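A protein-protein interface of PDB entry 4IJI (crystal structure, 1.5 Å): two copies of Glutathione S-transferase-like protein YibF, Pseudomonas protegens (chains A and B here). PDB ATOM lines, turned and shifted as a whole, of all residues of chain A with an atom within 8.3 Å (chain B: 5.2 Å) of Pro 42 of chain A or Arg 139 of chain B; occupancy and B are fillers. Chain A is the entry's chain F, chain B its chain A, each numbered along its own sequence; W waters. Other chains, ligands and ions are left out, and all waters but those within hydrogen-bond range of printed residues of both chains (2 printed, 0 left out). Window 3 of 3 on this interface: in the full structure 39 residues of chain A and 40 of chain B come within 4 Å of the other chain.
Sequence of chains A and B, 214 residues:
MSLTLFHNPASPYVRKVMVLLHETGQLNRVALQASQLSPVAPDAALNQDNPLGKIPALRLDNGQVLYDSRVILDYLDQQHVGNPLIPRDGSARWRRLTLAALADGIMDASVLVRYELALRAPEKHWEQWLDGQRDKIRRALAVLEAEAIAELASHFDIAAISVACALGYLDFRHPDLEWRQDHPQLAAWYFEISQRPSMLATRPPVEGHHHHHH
Among the printed residues, merely in contact across the chains: Pro 42 of chain A with Asp 135 of chain B (3.1 Å), Leu 52 of chain A with Arg 139 of chain B (3.4 Å), Pro 42 of chain A with Gly 132 of chain B (3.5 Å), Ala 41 of chain A with Gly 132 of chain B (3.6 Å), Leu 52 of chain A with Ala 140 of chain B (3.6 Å), Val 40 of chain A with Gly 132 of chain B (3.6 Å), Leu 52 of chain A with Val 143 of chain B (3.7 Å), Pro 42 of chain A with Lys 136 of chain B (3.7 Å) and Pro 42 of chain A with Arg 139 of chain B (3.9 Å).
Of the 11 printed residues of chain B, 6 touch a printed residue of chain A.
Printed residues of chain B that touch a printed residue of chain A: Gly 132, Asp 135, Lys 136, Arg 139, Ala 140 and Val 143.
Hydrophobic or aromatic side chains of chain B within 4 Å of the printed part of chain A: Val 143.
Printed residues of chain A that touch a printed residue of chain B: Val 40, Ala 41, Pro 42 and Leu 52.
Among the printed residues, 9 pairs touch across the chains.
NE of Arg 139 of chain B lies within salt-bridge range of OD2 of Asp 135 of chain B (2.4 Å).
Of the printed residues of chain B, Ala 41 of chain A touches Gly 132 (3.6 Å).
Pro 42 of chain A touches just these residues of chain B: Gly 132 (3.5 Å), Asp 135 (3.1 Å), Lys 136 (3.7 Å) and Arg 139 (3.9 Å).
Printed residues of chain B within 4 Å of Leu 52 of chain A: Arg 139, Ala 140 and Val 143.
Printed residues of chain A within 4 Å of Gly 132 of chain B: Val 40, Ala 41 and Pro 42.
Of chain A, only Leu 52 (3.6 Å) comes within 4 Å of Ala 140 of chain B.
Ala 142 of chain B touches none of the printed residues of chain A.
Of the printed residues of chain A, Val 143 of chain B touches Leu 52 (3.7 Å).
The nearest printed residue of chain B that does not touch Pro 42 of chain A is Arg 134 of chain B (6.9 Å).
The nearest residue of chain A that does not touch Arg 139 of chain B is Pro 51 of chain A (4.6 Å).
The nearest printed residue of chain B that does not touch Leu 52 of chain A is Lys 136 of chain B (5.1 Å).
Water W1 bridges NH1 of Arg 139 of chain B and O of Pro 51 of chain A.
Water W2 bridges the backbone carbonyl oxygen (O) of Ser 38 of chain A (3.1 Å) and the side-chain amino group (NZ) of Lys 136 of chain B (3.5 Å).
No position is printed for both chains.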
ATOM      1  N   GLN A  36     -35.859  22.801  19.915  1.00  0.00           N
ATOM      2  CA  GLN A  36     -36.672  22.526  18.741  1.00  0.00           C
ATOM      3  C   GLN A  36     -35.837  22.260  17.496  1.00  0.00           C
ATOM      4  O   GLN A  36     -34.906  23.006  17.191  1.00  0.00           O
ATOM      5  CB  GLN A  36     -37.630  23.697  18.487  1.00  0.00           C
ATOM      6  CG  GLN A  36     -36.970  25.093  18.440  1.00  0.00           C
ATOM      7  CD  GLN A  36     -36.516  25.616  19.810  1.00  0.00           C
ATOM      8  OE1 GLN A  36     -35.766  24.951  20.527  1.00  0.00           O
ATOM      9  NE2 GLN A  36     -36.967  26.813  20.167  1.00  0.00           N
ATOM     10  N   LEU A  37     -36.176  21.193  16.782  1.00  0.00           N
ATOM     11  CA  LEU A  37     -35.529  20.895  15.515  1.00  0.00           C
ATOM     12  C   LEU A  37     -36.126  21.781  14.429  1.00  0.00           C
ATOM     13  O   LEU A  37     -37.300  22.151  14.496  1.00  0.00           O
ATOM     14  CB  LEU A  37     -35.719  19.421  15.155  1.00  0.00           C
ATOM     15  CG  LEU A  37     -35.238  18.428  16.216  1.00  0.00           C
ATOM     16  CD1 LEU A  37     -35.598  16.992  15.842  1.00  0.00           C
ATOM     17  CD2 LEU A  37     -33.740  18.565  16.433  1.00  0.00           C
ATOM     18  N   SER A  38     -35.313  22.129  13.439  1.00  0.00           N
ATOM     19  CA  SER A  38     -35.785  22.908  12.294  1.00  0.00           C
ATOM     20  C   SER A  38     -35.123  22.420  11.010  1.00  0.00           C
ATOM     21  O   SER A  38     -34.423  23.176  10.339  1.00  0.00           O
ATOM     22  CB  SER A  38     -35.485  24.395  12.501  1.00  0.00           C
ATOM     23  OG  SER A  38     -34.085  24.633  12.564  1.00  0.00           O
ATOM     24  N   PRO A  39     -35.362  21.151  10.654  1.00  0.00           N
ATOM     25  CA  PRO A  39     -34.601  20.524   9.566  1.00  0.00           C
ATOM     26  C   PRO A  39     -34.935  21.074   8.174  1.00  0.00           C
ATOM     27  O   PRO A  39     -34.116  20.960   7.256  1.00  0.00           O
ATOM     28  CB  PRO A  39     -35.009  19.052   9.673  1.00  0.00           C
ATOM     29  CG  PRO A  39     -36.404  19.103  10.234  1.00  0.00           C
ATOM     30  CD  PRO A  39     -36.428  20.271  11.172  1.00  0.00           C
ATOM     31  N   VAL A  40     -36.120  21.655   8.013  1.00  0.00           N
ATOM     32  CA  VAL A  40     -36.507  22.225   6.724  1.00  0.00           C
ATOM     33  C   VAL A  40     -36.088  23.682   6.648  1.00  0.00           C
ATOM     34  O   VAL A  40     -35.391  24.088   5.718  1.00  0.00           O
ATOM     35  CB  VAL A  40     -38.022  22.108   6.468  1.00  0.00           C
ATOM     36  CG1 VAL A  40     -38.373  22.695   5.114  1.00  0.00           C
ATOM     37  CG2 VAL A  40     -38.450  20.661   6.541  1.00  0.00           C
ATOM     38  N   ALA A  41     -36.511  24.460   7.641  1.00  0.00           N
ATOM     39  CA  ALA A  41     -36.158  25.871   7.742  1.00  0.00           C
ATOM     40  C   ALA A  41     -36.257  26.312   9.195  1.00  0.00           C
ATOM     41  O   ALA A  41     -37.153  25.872   9.914  1.00  0.00           O
ATOM     42  CB  ALA A  41     -37.090  26.703   6.891  1.00  0.00           C
ATOM     43  N   PRO A  42     -35.335  27.178   9.642  1.00  0.00           N
ATOM     44  CA  PRO A  42     -35.506  27.714  10.996  1.00  0.00           C
ATOM     45  C   PRO A  42     -36.505  28.863  11.018  1.00  0.00           C
ATOM     46  O   PRO A  42     -37.559  28.715  11.629  1.00  0.00           O
ATOM     47  CB  PRO A  42     -34.105  28.212  11.355  1.00  0.00           C
ATOM     48  CG  PRO A  42     -33.475  28.531  10.054  1.00  0.00           C
ATOM     49  CD  PRO A  42     -34.037  27.557   9.052  1.00  0.00           C
ATOM     50  N   ASN A  50     -29.024  30.537  22.546  1.00  0.00           N
ATOM     51  CA  ASN A  50     -28.721  29.649  21.422  1.00  0.00           C
ATOM     52  C   ASN A  50     -29.299  30.178  20.112  1.00  0.00           C
ATOM     53  O   ASN A  50     -30.172  29.542  19.526  1.00  0.00           O
ATOM     54  CB  ASN A  50     -29.258  28.245  21.718  1.00  0.00           C
ATOM     55  CG  ASN A  50     -28.684  27.179  20.792  1.00  0.00           C
ATOM     56  OD1 ASN A  50     -27.737  27.419  20.040  1.00  0.00           O
ATOM     57  ND2 ASN A  50     -29.264  25.987  20.850  1.00  0.00           N
ATOM     58  N   PRO A  51     -28.795  31.335  19.639  1.00  0.00           N
ATOM     59  CA  PRO A  51     -29.396  32.032  18.492  1.00  0.00           C
ATOM     60  C   PRO A  51     -29.325  31.257  17.187  1.00  0.00           C
ATOM     61  O   PRO A  51     -30.146  31.496  16.297  1.00  0.00           O
ATOM     62  CB  PRO A  51     -28.555  33.314  18.382  1.00  0.00           C
ATOM     63  CG  PRO A  51     -27.246  32.960  19.022  1.00  0.00           C
ATOM     64  CD  PRO A  51     -27.634  32.070  20.166  1.00  0.00           C
ATOM     65  N   LEU A  52     -28.358  30.346  17.063  1.00  0.00           N
ATOM     66  CA  LEU A  52     -28.197  29.578  15.833  1.00  0.00           C
ATOM     67  C   LEU A  52     -28.907  28.231  15.922  1.00  0.00           C
ATOM     68  O   LEU A  52     -28.883  27.440  14.970  1.00  0.00           O
ATOM     69  CB  LEU A  52     -26.711  29.364  15.520  1.00  0.00           C
ATOM     70  CG  LEU A  52     -25.889  30.628  15.278  1.00  0.00           C
ATOM     71  CD1 LEU A  52     -24.509  30.253  14.809  1.00  0.00           C
ATOM     72  CD2 LEU A  52     -26.570  31.526  14.254  1.00  0.00           C
ATOM     73  N   GLY A  53     -29.553  27.986  17.061  1.00  0.00           N
ATOM     74  CA  GLY A  53     -30.280  26.743  17.263  1.00  0.00           C
ATOM     75  C   GLY A  53     -29.419  25.506  17.076  1.00  0.00           C
ATOM     76  O   GLY A  53     -29.855  24.498  16.504  1.00  0.00           O
ATOM     77  N   TYR A  67     -20.349  24.407  20.622  1.00  0.00           N
ATOM     78  CA  TYR A  67     -20.896  23.456  19.660  1.00  0.00           C
ATOM     79  C   TYR A  67     -19.773  23.246  18.631  1.00  0.00           C
ATOM     80  O   TYR A  67     -18.801  24.014  18.651  1.00  0.00           O
ATOM     81  CB  TYR A  67     -22.190  24.015  19.031  1.00  0.00           C
ATOM     82  CG  TYR A  67     -22.044  25.390  18.451  1.00  0.00           C
ATOM     83  CD1 TYR A  67     -21.485  25.571  17.194  1.00  0.00           C
ATOM     84  CD2 TYR A  67     -22.471  26.514  19.160  1.00  0.00           C
ATOM     85  CE1 TYR A  67     -21.341  26.827  16.656  1.00  0.00           C
ATOM     86  CE2 TYR A  67     -22.333  27.782  18.610  1.00  0.00           C
ATOM     87  CZ  TYR A  67     -21.757  27.924  17.364  1.00  0.00           C
ATOM     88  OH  TYR A  67     -21.597  29.181  16.795  1.00  0.00           O
ATOM     89  N   GLY B 132     -34.449  27.682   3.954  1.00  0.00           N
ATOM     90  CA  GLY B 132     -33.960  27.370   5.285  1.00  0.00           C
ATOM     91  C   GLY B 132     -32.450  27.448   5.393  1.00  0.00           C
ATOM     92  O   GLY B 132     -31.919  28.008   6.355  1.00  0.00           O
ATOM     93  N   ARG B 134     -30.377  29.064   3.347  1.00  0.00           N
ATOM     94  CA  ARG B 134     -30.026  30.470   3.149  1.00  0.00           C
ATOM     95  C   ARG B 134     -30.109  31.225   4.481  1.00  0.00           C
ATOM     96  O   ARG B 134     -29.193  31.962   4.860  1.00  0.00           O
ATOM     97  CB  ARG B 134     -30.965  31.091   2.108  1.00  0.00           C
ATOM     98  CG  ARG B 134     -30.419  32.314   1.392  1.00  0.00           C
ATOM     99  CD  ARG B 134     -31.338  32.754   0.242  1.00  0.00           C
ATOM    100  NE  ARG B 134     -31.535  31.703  -0.757  1.00  0.00           N
ATOM    101  CZ  ARG B 134     -32.697  31.099  -0.995  1.00  0.00           C
ATOM    102  NH1 ARG B 134     -32.781  30.149  -1.918  1.00  0.00           N
ATOM    103  NH2 ARG B 134     -33.778  31.442  -0.311  1.00  0.00           N
ATOM    104  N   ASP B 135     -31.204  31.012   5.203  1.00  0.00           N
ATOM    105  CA  ASP B 135     -31.408  31.648   6.495  1.00  0.00           C
ATOM    106  C   ASP B 135     -30.386  31.186   7.533  1.00  0.00           C
ATOM    107  O   ASP B 135     -29.866  31.997   8.296  1.00  0.00           O
ATOM    108  CB  ASP B 135     -32.832  31.391   7.000  1.00  0.00           C
ATOM    109  CG  ASP B 135     -33.147  32.170   8.262  1.00  0.00           C
ATOM    110  OD1 ASP B 135     -33.317  33.406   8.176  1.00  0.00           O
ATOM    111  OD2 ASP B 135     -33.218  31.547   9.337  1.00  0.00           O
ATOM    112  N   LYS B 136     -30.086  29.891   7.568  1.00  0.00           N
ATOM    113  CA  LYS B 136     -29.120  29.378   8.537  1.00  0.00           C
ATOM    114  C   LYS B 136     -27.738  29.994   8.330  1.00  0.00           C
ATOM    115  O   LYS B 136     -27.013  30.284   9.288  1.00  0.00           O
ATOM    116  CB  LYS B 136     -29.045  27.848   8.481  1.00  0.00           C
ATOM    117  CG  LYS B 136     -30.131  27.147   9.289  1.00  0.00           C
ATOM    118  CD  LYS B 136     -30.373  25.727   8.791  1.00  0.00           C
ATOM    119  CE  LYS B 136     -29.117  24.874   8.864  1.00  0.00           C
ATOM    120  NZ  LYS B 136     -29.380  23.482   8.392  1.00  0.00           N
ATOM    121  N   ILE B 137     -27.376  30.183   7.070  1.00  0.00           N
ATOM    122  CA  ILE B 137     -26.098  30.790   6.747  1.00  0.00           C
ATOM    123  C   ILE B 137     -26.108  32.249   7.179  1.00  0.00           C
ATOM    124  O   ILE B 137     -25.162  32.727   7.806  1.00  0.00           O
ATOM    125  CB  ILE B 137     -25.803  30.647   5.241  1.00  0.00           C
ATOM    126  CG1 ILE B 137     -25.468  29.185   4.922  1.00  0.00           C
ATOM    127  CG2 ILE B 137     -24.667  31.570   4.819  1.00  0.00           C
ATOM    128  CD1 ILE B 137     -25.518  28.876   3.444  1.00  0.00           C
ATOM    129  N   ARG B 138     -27.187  32.955   6.867  1.00  0.00           N
ATOM    130  CA  ARG B 138     -27.279  34.367   7.238  1.00  0.00           C
ATOM    131  C   ARG B 138     -27.219  34.587   8.738  1.00  0.00           C
ATOM    132  O   ARG B 138     -26.562  35.519   9.206  1.00  0.00           O
ATOM    133  CB  ARG B 138     -28.572  34.976   6.687  1.00  0.00           C
ATOM    134  CG  ARG B 138     -28.495  35.325   5.220  1.00  0.00           C
ATOM    135  CD  ARG B 138     -29.868  35.649   4.682  1.00  0.00           C
ATOM    136  NE  ARG B 138     -29.812  35.917   3.252  1.00  0.00           N
ATOM    137  CZ  ARG B 138     -30.841  35.763   2.429  1.00  0.00           C
ATOM    138  NH1 ARG B 138     -32.008  35.334   2.898  1.00  0.00           N
ATOM    139  NH2 ARG B 138     -30.701  36.030   1.139  1.00  0.00           N
ATOM    140  N   ARG B 139     -27.889  33.725   9.499  1.00  0.00           N
ATOM    141  CA  ARG B 139     -27.874  33.878  10.956  1.00  0.00           C
ATOM    142  C   ARG B 139     -26.476  33.660  11.527  1.00  0.00           C
ATOM    143  O   ARG B 139     -26.045  34.361  12.456  1.00  0.00           O
ATOM    144  CB  ARG B 139     -28.895  32.947  11.623  1.00  0.00           C
ATOM    145  CG  ARG B 139     -30.338  33.312  11.313  1.00  0.00           C
ATOM    146  CD  ARG B 139     -31.324  32.371  11.988  1.00  0.00           C
ATOM    147  NE  ARG B 139     -32.680  32.572  11.474  1.00  0.00           N
ATOM    148  CZ  ARG B 139     -33.790  32.199  12.105  1.00  0.00           C
ATOM    149  NH1 ARG B 139     -33.725  31.605  13.285  1.00  0.00           N
ATOM    150  NH2 ARG B 139     -34.971  32.431  11.549  1.00  0.00           N
ATOM    151  N   ALA B 140     -25.750  32.709  10.956  1.00  0.00           N
ATOM    152  CA  ALA B 140     -24.393  32.448  11.399  1.00  0.00           C
ATOM    153  C   ALA B 140     -23.489  33.645  11.122  1.00  0.00           C
ATOM    154  O   ALA B 140     -22.660  34.020  11.951  1.00  0.00           O
ATOM    155  CB  ALA B 140     -23.852  31.208  10.729  1.00  0.00           C
ATOM    156  N   LEU B 141     -23.639  34.229   9.939  1.00  0.00           N
ATOM    157  CA  LEU B 141     -22.874  35.419   9.582  1.00  0.00           C
ATOM    158  C   LEU B 141     -23.205  36.567  10.520  1.00  0.00           C
ATOM    159  O   LEU B 141     -22.327  37.332  10.915  1.00  0.00           O
ATOM    160  CB  LEU B 141     -23.157  35.825   8.136  1.00  0.00           C
ATOM    161  CG  LEU B 141     -22.695  34.840   7.060  1.00  0.00           C
ATOM    162  CD1 LEU B 141     -23.294  35.202   5.707  1.00  0.00           C
ATOM    163  CD2 LEU B 141     -21.174  34.795   6.981  1.00  0.00           C
ATOM    164  N   ALA B 142     -24.479  36.701  10.872  1.00  0.00           N
ATOM    165  CA  ALA B 142     -24.885  37.776  11.769  1.00  0.00           C
ATOM    166  C   ALA B 142     -24.239  37.626  13.140  1.00  0.00           C
ATOM    167  O   ALA B 142     -23.884  38.609  13.779  1.00  0.00           O
ATOM    168  CB  ALA B 142     -26.404  37.834  11.904  1.00  0.00           C
ATOM    169  N   VAL B 143     -24.098  36.391  13.607  1.00  0.00           N
ATOM    170  CA  VAL B 143     -23.423  36.153  14.876  1.00  0.00           C
ATOM    171  C   VAL B 143     -21.950  36.539  14.794  1.00  0.00           C
ATOM    172  O   VAL B 143     -21.416  37.190  15.698  1.00  0.00           O
ATOM    173  CB  VAL B 143     -23.575  34.687  15.317  1.00  0.00           C
ATOM    174  CG1 VAL B 143     -22.576  34.358  16.423  1.00  0.00           C
ATOM    175  CG2 VAL B 143     -24.998  34.446  15.806  1.00  0.00           C
HETATM  176  O   HOH W   1     -31.777  30.203  14.489  1.00  0.00           O
HETATM  177  O   HOH W   2     -31.531  22.005  10.682  1.00  0.00           O
